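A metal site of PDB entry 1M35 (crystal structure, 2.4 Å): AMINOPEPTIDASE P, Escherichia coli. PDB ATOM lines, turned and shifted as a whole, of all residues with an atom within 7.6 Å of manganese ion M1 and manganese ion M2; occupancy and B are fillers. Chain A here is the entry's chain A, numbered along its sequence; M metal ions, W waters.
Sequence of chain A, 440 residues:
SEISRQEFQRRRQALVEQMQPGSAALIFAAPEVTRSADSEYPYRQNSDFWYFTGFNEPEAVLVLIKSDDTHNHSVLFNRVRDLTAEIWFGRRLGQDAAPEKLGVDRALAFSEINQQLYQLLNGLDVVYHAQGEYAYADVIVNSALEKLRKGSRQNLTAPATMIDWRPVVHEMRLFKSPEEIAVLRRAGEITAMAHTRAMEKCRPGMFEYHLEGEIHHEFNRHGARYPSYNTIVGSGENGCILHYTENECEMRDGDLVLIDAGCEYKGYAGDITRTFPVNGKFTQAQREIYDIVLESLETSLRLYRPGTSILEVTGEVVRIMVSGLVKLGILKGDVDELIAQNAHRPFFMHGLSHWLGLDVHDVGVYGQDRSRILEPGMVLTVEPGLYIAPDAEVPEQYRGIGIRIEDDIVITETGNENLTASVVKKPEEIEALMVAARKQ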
ATOM      1  N   TYR A 229      31.946  26.237 -35.220  1.00  0.00           N
ATOM      2  CA  TYR A 229      30.718  26.445 -35.977  1.00  0.00           C
ATOM      3  C   TYR A 229      30.776  27.847 -36.557  1.00  0.00           C
ATOM      4  O   TYR A 229      31.606  28.658 -36.144  1.00  0.00           O
ATOM      5  CB  TYR A 229      29.466  26.308 -35.101  1.00  0.00           C
ATOM      6  CG  TYR A 229      29.465  27.181 -33.870  1.00  0.00           C
ATOM      7  CD1 TYR A 229      30.126  26.777 -32.697  1.00  0.00           C
ATOM      8  CD2 TYR A 229      28.843  28.431 -33.878  1.00  0.00           C
ATOM      9  CE1 TYR A 229      30.154  27.593 -31.559  1.00  0.00           C
ATOM     10  CE2 TYR A 229      28.862  29.261 -32.745  1.00  0.00           C
ATOM     11  CZ  TYR A 229      29.522  28.830 -31.585  1.00  0.00           C
ATOM     12  OH  TYR A 229      29.550  29.637 -30.473  1.00  0.00           O
ATOM     13  N   ILE A 232      28.309  33.911 -35.454  1.00  0.00           N
ATOM     14  CA  ILE A 232      27.111  34.717 -35.589  1.00  0.00           C
ATOM     15  C   ILE A 232      27.339  36.088 -34.958  1.00  0.00           C
ATOM     16  O   ILE A 232      27.722  36.180 -33.781  1.00  0.00           O
ATOM     17  CB  ILE A 232      25.919  34.061 -34.890  1.00  0.00           C
ATOM     18  CG1 ILE A 232      25.560  32.759 -35.599  1.00  0.00           C
ATOM     19  CG2 ILE A 232      24.736  35.012 -34.843  1.00  0.00           C
ATOM     20  CD1 ILE A 232      24.476  31.972 -34.876  1.00  0.00           C
ATOM     21  N   ILE A 259      26.547  38.091 -30.249  1.00  0.00           N
ATOM     22  CA  ILE A 259      27.646  37.325 -30.803  1.00  0.00           C
ATOM     23  C   ILE A 259      27.710  35.916 -30.250  1.00  0.00           C
ATOM     24  O   ILE A 259      27.896  35.721 -29.049  1.00  0.00           O
ATOM     25  CB  ILE A 259      29.011  37.987 -30.529  1.00  0.00           C
ATOM     26  CG1 ILE A 259      29.050  39.395 -31.141  1.00  0.00           C
ATOM     27  CG2 ILE A 259      30.133  37.138 -31.099  1.00  0.00           C
ATOM     28  CD1 ILE A 259      30.381  40.100 -30.927  1.00  0.00           C
ATOM     29  N   ASP A 260      27.536  34.933 -31.136  1.00  0.00           N
ATOM     30  CA  ASP A 260      27.618  33.538 -30.753  1.00  0.00           C
ATOM     31  C   ASP A 260      28.795  32.982 -31.545  1.00  0.00           C
ATOM     32  O   ASP A 260      28.735  32.892 -32.772  1.00  0.00           O
ATOM     33  CB  ASP A 260      26.331  32.796 -31.125  1.00  0.00           C
ATOM     34  CG  ASP A 260      26.242  31.424 -30.467  1.00  0.00           C
ATOM     35  OD1 ASP A 260      27.294  30.877 -30.087  1.00  0.00           O
ATOM     36  OD2 ASP A 260      25.125  30.888 -30.349  1.00  0.00           O
ATOM     37  N   ALA A 261      29.873  32.647 -30.849  1.00  0.00           N
ATOM     38  CA  ALA A 261      31.058  32.124 -31.503  1.00  0.00           C
ATOM     39  C   ALA A 261      31.824  31.219 -30.551  1.00  0.00           C
ATOM     40  O   ALA A 261      31.815  31.432 -29.337  1.00  0.00           O
ATOM     41  CB  ALA A 261      31.942  33.265 -31.962  1.00  0.00           C
ATOM     42  N   GLY A 262      32.469  30.202 -31.118  1.00  0.00           N
ATOM     43  CA  GLY A 262      33.228  29.264 -30.327  1.00  0.00           C
ATOM     44  C   GLY A 262      34.367  28.706 -31.156  1.00  0.00           C
ATOM     45  O   GLY A 262      34.245  28.500 -32.366  1.00  0.00           O
ATOM     46  N   GLY A 270      34.076  25.205 -28.144  1.00  0.00           N
ATOM     47  CA  GLY A 270      33.722  26.183 -27.148  1.00  0.00           C
ATOM     48  C   GLY A 270      32.426  26.705 -27.761  1.00  0.00           C
ATOM     49  O   GLY A 270      32.254  26.597 -28.983  1.00  0.00           O
ATOM     50  N   ASP A 271      31.517  27.237 -26.958  1.00  0.00           N
ATOM     51  CA  ASP A 271      30.257  27.743 -27.498  1.00  0.00           C
ATOM     52  C   ASP A 271      29.755  28.828 -26.563  1.00  0.00           C
ATOM     53  O   ASP A 271      29.097  28.545 -25.563  1.00  0.00           O
ATOM     54  CB  ASP A 271      29.217  26.608 -27.627  1.00  0.00           C
ATOM     55  CG  ASP A 271      27.864  27.077 -28.191  1.00  0.00           C
ATOM     56  OD1 ASP A 271      27.734  28.233 -28.627  1.00  0.00           O
ATOM     57  OD2 ASP A 271      26.908  26.261 -28.206  1.00  0.00           O
ATOM     58  N   ILE A 272      30.090  30.078 -26.892  1.00  0.00           N
ATOM     59  CA  ILE A 272      29.697  31.210 -26.071  1.00  0.00           C
ATOM     60  C   ILE A 272      28.842  32.234 -26.795  1.00  0.00           C
ATOM     61  O   ILE A 272      29.053  32.501 -27.973  1.00  0.00           O
ATOM     62  CB  ILE A 272      30.939  31.977 -25.534  1.00  0.00           C
ATOM     63  CG1 ILE A 272      31.717  31.115 -24.537  1.00  0.00           C
ATOM     64  CG2 ILE A 272      30.510  33.307 -24.887  1.00  0.00           C
ATOM     65  CD1 ILE A 272      32.943  31.835 -23.925  1.00  0.00           C
ATOM     66  N   THR A 273      27.880  32.805 -26.089  1.00  0.00           N
ATOM     67  CA  THR A 273      27.062  33.855 -26.665  1.00  0.00           C
ATOM     68  C   THR A 273      27.056  35.009 -25.668  1.00  0.00           C
ATOM     69  O   THR A 273      26.890  34.805 -24.467  1.00  0.00           O
ATOM     70  CB  THR A 273      25.590  33.463 -26.908  1.00  0.00           C
ATOM     71  OG1 THR A 273      25.505  32.337 -27.788  1.00  0.00           O
ATOM     72  CG2 THR A 273      24.855  34.626 -27.545  1.00  0.00           C
ATOM     73  N   GLY A 351      15.927  25.443 -27.278  1.00  0.00           N
ATOM     74  CA  GLY A 351      16.249  24.770 -26.028  1.00  0.00           C
ATOM     75  C   GLY A 351      17.179  25.565 -25.137  1.00  0.00           C
ATOM     76  O   GLY A 351      17.891  26.465 -25.603  1.00  0.00           O
ATOM     77  N   LEU A 352      17.198  25.220 -23.855  1.00  0.00           N
ATOM     78  CA  LEU A 352      18.045  25.901 -22.903  1.00  0.00           C
ATOM     79  C   LEU A 352      19.465  25.356 -22.947  1.00  0.00           C
ATOM     80  O   LEU A 352      20.429  26.102 -22.766  1.00  0.00           O
ATOM     81  CB  LEU A 352      17.492  25.735 -21.493  1.00  0.00           C
ATOM     82  CG  LEU A 352      18.301  26.395 -20.376  1.00  0.00           C
ATOM     83  CD1 LEU A 352      18.271  27.909 -20.532  1.00  0.00           C
ATOM     84  CD2 LEU A 352      17.717  25.970 -19.027  1.00  0.00           C
ATOM     85  N   SER A 353      19.600  24.052 -23.194  1.00  0.00           N
ATOM     86  CA  SER A 353      20.910  23.418 -23.201  1.00  0.00           C
ATOM     87  C   SER A 353      21.089  22.284 -24.197  1.00  0.00           C
ATOM     88  O   SER A 353      20.129  21.607 -24.567  1.00  0.00           O
ATOM     89  CB  SER A 353      21.215  22.833 -21.811  1.00  0.00           C
ATOM     90  OG  SER A 353      21.059  23.794 -20.785  1.00  0.00           O
ATOM     91  N   HIS A 354      22.334  22.082 -24.625  1.00  0.00           N
ATOM     92  CA  HIS A 354      22.683  20.984 -25.512  1.00  0.00           C
ATOM     93  C   HIS A 354      24.046  20.459 -25.084  1.00  0.00           C
ATOM     94  O   HIS A 354      24.845  21.220 -24.520  1.00  0.00           O
ATOM     95  CB  HIS A 354      22.681  21.433 -26.987  1.00  0.00           C
ATOM     96  CG  HIS A 354      23.702  22.478 -27.314  1.00  0.00           C
ATOM     97  ND1 HIS A 354      25.061  22.265 -27.348  1.00  0.00           N
ATOM     98  CD2 HIS A 354      23.530  23.777 -27.673  1.00  0.00           C
ATOM     99  CE1 HIS A 354      25.659  23.411 -27.707  1.00  0.00           C
ATOM    100  NE2 HIS A 354      24.778  24.363 -27.912  1.00  0.00           N
ATOM    101  N   TRP A 355      24.301  19.171 -25.291  1.00  0.00           N
ATOM    102  CA  TRP A 355      25.590  18.580 -24.924  1.00  0.00           C
ATOM    103  C   TRP A 355      26.690  19.307 -25.686  1.00  0.00           C
ATOM    104  O   TRP A 355      26.442  19.890 -26.739  1.00  0.00           O
ATOM    105  CB  TRP A 355      25.642  17.089 -25.278  1.00  0.00           C
ATOM    106  CG  TRP A 355      24.519  16.226 -24.739  1.00  0.00           C
ATOM    107  CD1 TRP A 355      23.747  15.362 -25.462  1.00  0.00           C
ATOM    108  CD2 TRP A 355      24.074  16.122 -23.380  1.00  0.00           C
ATOM    109  NE1 TRP A 355      22.844  14.725 -24.640  1.00  0.00           N
ATOM    110  CE2 TRP A 355      23.024  15.170 -23.356  1.00  0.00           C
ATOM    111  CE3 TRP A 355      24.453  16.736 -22.176  1.00  0.00           C
ATOM    112  CZ2 TRP A 355      22.353  14.823 -22.176  1.00  0.00           C
ATOM    113  CZ3 TRP A 355      23.783  16.393 -21.006  1.00  0.00           C
ATOM    114  CH2 TRP A 355      22.744  15.445 -21.012  1.00  0.00           C
ATOM    115  N   LEU A 356      27.921  19.252 -25.177  1.00  0.00           N
ATOM    116  CA  LEU A 356      29.049  19.897 -25.820  1.00  0.00           C
ATOM    117  C   LEU A 356      30.249  18.950 -25.786  1.00  0.00           C
ATOM    118  O   LEU A 356      30.459  18.252 -24.791  1.00  0.00           O
ATOM    119  CB  LEU A 356      29.388  21.201 -25.090  1.00  0.00           C
ATOM    120  CG  LEU A 356      30.457  22.103 -25.703  1.00  0.00           C
ATOM    121  CD1 LEU A 356      29.920  22.714 -27.000  1.00  0.00           C
ATOM    122  CD2 LEU A 356      30.838  23.204 -24.722  1.00  0.00           C
ATOM    123  N   VAL A 360      29.866  20.799 -31.492  1.00  0.00           N
ATOM    124  CA  VAL A 360      29.204  21.829 -30.719  1.00  0.00           C
ATOM    125  C   VAL A 360      27.861  21.318 -30.185  1.00  0.00           C
ATOM    126  O   VAL A 360      27.518  21.584 -29.030  1.00  0.00           O
ATOM    127  CB  VAL A 360      29.053  23.152 -31.521  1.00  0.00           C
ATOM    128  CG1 VAL A 360      28.178  22.942 -32.750  1.00  0.00           C
ATOM    129  CG2 VAL A 360      28.460  24.236 -30.616  1.00  0.00           C
ATOM    130  N   HIS A 361      27.107  20.603 -31.013  1.00  0.00           N
ATOM    131  CA  HIS A 361      25.840  19.990 -30.599  1.00  0.00           C
ATOM    132  C   HIS A 361      26.247  18.532 -30.453  1.00  0.00           C
ATOM    133  O   HIS A 361      26.009  17.721 -31.340  1.00  0.00           O
ATOM    134  CB  HIS A 361      24.781  20.134 -31.685  1.00  0.00           C
ATOM    135  CG  HIS A 361      24.289  21.537 -31.842  1.00  0.00           C
ATOM    136  ND1 HIS A 361      23.547  21.976 -32.916  1.00  0.00           N
ATOM    137  CD2 HIS A 361      24.444  22.616 -31.034  1.00  0.00           C
ATOM    138  CE1 HIS A 361      23.284  23.282 -32.723  1.00  0.00           C
ATOM    139  NE2 HIS A 361      23.820  23.711 -31.595  1.00  0.00           N
ATOM    140  N   LEU A 380      27.551  20.569 -20.973  1.00  0.00           N
ATOM    141  CA  LEU A 380      26.447  21.157 -21.705  1.00  0.00           C
ATOM    142  C   LEU A 380      26.490  22.676 -21.674  1.00  0.00           C
ATOM    143  O   LEU A 380      27.216  23.276 -20.882  1.00  0.00           O
ATOM    144  CB  LEU A 380      25.106  20.710 -21.096  1.00  0.00           C
ATOM    145  CG  LEU A 380      24.917  21.047 -19.604  1.00  0.00           C
ATOM    146  CD1 LEU A 380      23.436  21.152 -19.264  1.00  0.00           C
ATOM    147  CD2 LEU A 380      25.602  19.990 -18.742  1.00  0.00           C
ATOM    148  N   THR A 381      25.695  23.293 -22.534  1.00  0.00           N
ATOM    149  CA  THR A 381      25.626  24.740 -22.591  1.00  0.00           C
ATOM    150  C   THR A 381      24.390  25.193 -21.830  1.00  0.00           C
ATOM    151  O   THR A 381      23.512  24.391 -21.497  1.00  0.00           O
ATOM    152  CB  THR A 381      25.478  25.256 -24.046  1.00  0.00           C
ATOM    153  OG1 THR A 381      24.269  24.746 -24.612  1.00  0.00           O
ATOM    154  CG2 THR A 381      26.667  24.806 -24.897  1.00  0.00           C
ATOM    155  N   VAL A 382      24.342  26.481 -21.517  1.00  0.00           N
ATOM    156  CA  VAL A 382      23.203  27.076 -20.836  1.00  0.00           C
ATOM    157  C   VAL A 382      23.006  28.346 -21.634  1.00  0.00           C
ATOM    158  O   VAL A 382      23.798  29.287 -21.507  1.00  0.00           O
ATOM    159  CB  VAL A 382      23.527  27.421 -19.366  1.00  0.00           C
ATOM    160  CG1 VAL A 382      22.256  27.804 -18.641  1.00  0.00           C
ATOM    161  CG2 VAL A 382      24.208  26.232 -18.689  1.00  0.00           C
ATOM    162  N   GLU A 383      21.966  28.380 -22.448  1.00  0.00           N
ATOM    163  CA  GLU A 383      21.772  29.549 -23.294  1.00  0.00           C
ATOM    164  C   GLU A 383      20.380  30.113 -23.405  1.00  0.00           C
ATOM    165  O   GLU A 383      19.754  30.057 -24.462  1.00  0.00           O
ATOM    166  CB  GLU A 383      22.323  29.244 -24.695  1.00  0.00           C
ATOM    167  CG  GLU A 383      21.829  27.943 -25.316  1.00  0.00           C
ATOM    168  CD  GLU A 383      22.580  27.563 -26.592  1.00  0.00           C
ATOM    169  OE1 GLU A 383      22.579  28.373 -27.550  1.00  0.00           O
ATOM    170  OE2 GLU A 383      23.178  26.476 -26.642  1.00  0.00           O
ATOM    171  N   ARG A 404      20.730  36.886 -26.123  1.00  0.00           N
ATOM    172  CA  ARG A 404      21.056  35.547 -25.682  1.00  0.00           C
ATOM    173  C   ARG A 404      22.379  35.617 -24.939  1.00  0.00           C
ATOM    174  O   ARG A 404      23.284  36.352 -25.345  1.00  0.00           O
ATOM    175  CB  ARG A 404      21.166  34.575 -26.861  1.00  0.00           C
ATOM    176  CG  ARG A 404      21.598  33.185 -26.424  1.00  0.00           C
ATOM    177  CD  ARG A 404      21.371  32.092 -27.467  1.00  0.00           C
ATOM    178  NE  ARG A 404      22.285  32.153 -28.597  1.00  0.00           N
ATOM    179  CZ  ARG A 404      21.952  32.617 -29.804  1.00  0.00           C
ATOM    180  NH1 ARG A 404      20.723  33.048 -30.032  1.00  0.00           N
ATOM    181  NH2 ARG A 404      22.854  32.614 -30.776  1.00  0.00           N
ATOM    182  N   GLU A 406      25.141  32.862 -23.263  1.00  0.00           N
ATOM    183  CA  GLU A 406      25.433  31.441 -23.175  1.00  0.00           C
ATOM    184  C   GLU A 406      26.804  31.073 -22.593  1.00  0.00           C
ATOM    185  O   GLU A 406      27.814  31.629 -22.989  1.00  0.00           O
ATOM    186  CB  GLU A 406      25.282  30.817 -24.576  1.00  0.00           C
ATOM    187  CG  GLU A 406      25.964  29.464 -24.802  1.00  0.00           C
ATOM    188  CD  GLU A 406      25.730  28.910 -26.221  1.00  0.00           C
ATOM    189  OE1 GLU A 406      25.778  29.702 -27.194  1.00  0.00           O
ATOM    190  OE2 GLU A 406      25.525  27.679 -26.361  1.00  0.00           O
ATOM    191  N   ASP A 407      26.804  30.147 -21.648  1.00  0.00           N
ATOM    192  CA  ASP A 407      28.032  29.658 -21.024  1.00  0.00           C
ATOM    193  C   ASP A 407      28.105  28.145 -21.199  1.00  0.00           C
ATOM    194  O   ASP A 407      27.095  27.500 -21.491  1.00  0.00           O
ATOM    195  CB  ASP A 407      28.071  29.970 -19.515  1.00  0.00           C
ATOM    196  CG  ASP A 407      28.526  31.384 -19.212  1.00  0.00           C
ATOM    197  OD1 ASP A 407      29.378  31.927 -19.949  1.00  0.00           O
ATOM    198  OD2 ASP A 407      28.045  31.951 -18.201  1.00  0.00           O
ATOM    199  N   ASP A 408      29.304  27.591 -21.010  1.00  0.00           N
ATOM    200  CA  ASP A 408      29.503  26.157 -21.136  1.00  0.00           C
ATOM    201  C   ASP A 408      29.884  25.637 -19.753  1.00  0.00           C
ATOM    202  O   ASP A 408      30.783  26.198 -19.110  1.00  0.00           O
ATOM    203  CB  ASP A 408      30.628  25.828 -22.135  1.00  0.00           C
ATOM    204  CG  ASP A 408      30.453  26.541 -23.465  1.00  0.00           C
ATOM    205  OD1 ASP A 408      29.286  26.798 -23.872  1.00  0.00           O
ATOM    206  OD2 ASP A 408      31.470  26.836 -24.129  1.00  0.00           O
HETATM  207 MN    MN M   1      24.978  26.459 -27.992  1.00  0.00          MN
HETATM  208 MN    MN M   2      26.061  29.130 -29.269  1.00  0.00          MN
HETATM  209  O   HOH W   1      24.410  27.896 -29.196  1.00  0.00           O
HETATM  210  O   HOH W   2      26.309  27.940 -31.375  1.00  0.00           O
HETATM  211  O   HOH W   3      23.878  26.567 -31.177  1.00  0.00           O
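Residues that only touch manganese ion M2: Tyr 229 (3.7 Å) and Thr 273 (3.6 Å).
Manganese ion M2 is bound by the side-chain carboxylate (OD1) of Asp 271, water W1, the side-chain carboxylate (OE1) of Glu 406, the side-chain carboxylate (OD2) of Asp 260, the side-chain carboxylate (OD1) of Asp 260 and water W2.
Merely in contact with manganese ion M1: Thr 381. The nearest printed residue that does not touch manganese ion M1 is His 361 (4.7 Å).
The side-chain carboxylate (OD1) of Asp 271 sits close to the side-chain hydroxyl (OH) of Tyr 229 (2.9 Å). The backbone carbonyl oxygen of Thr 273 sits at hydrogen-bond distance from the backbone NH of Glu 406 (2.9 Å). The side-chain hydroxyl (OG1) of Thr 381 lies close to the side-chain carboxylate (OE2) of Glu 383, at 2.9 Å. The side-chain carboxylate of Glu 383 is in salt-bridge range of the guanidinium group of Arg 404 (3.9 Å). The backbone carbonyl oxygen of Leu 352 lies within hydrogen-bond range of the backbone NH of Glu 383. The side-chain carboxylate (OD2) of Asp 260 sits close to the guanidinium group (NH2) of Arg 404, 2.9 Å away. The guanidinium group (NE) of Arg 404 is in hydrogen-bond range of the side-chain hydroxyl (OG1) of Thr 273 (3.3 Å). N of Gly 262 is in hydrogen-bond range of OH of Tyr 229 (3.0 Å).
Manganese ion M1 is bound by OD2 of Asp 271 (2.0 Å). Manganese ion M1 is bound by water W1, 2.0 Å away. A ring nitrogen (NE2) of His 354 binds manganese ion M1, 2.1 Å away. The side-chain carboxylate (OE2) of Glu 406 binds manganese ion M1, at 2.1 Å. The side-chain carboxylate (OE2) of Glu 383 binds manganese ion M1 (2.3 Å).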
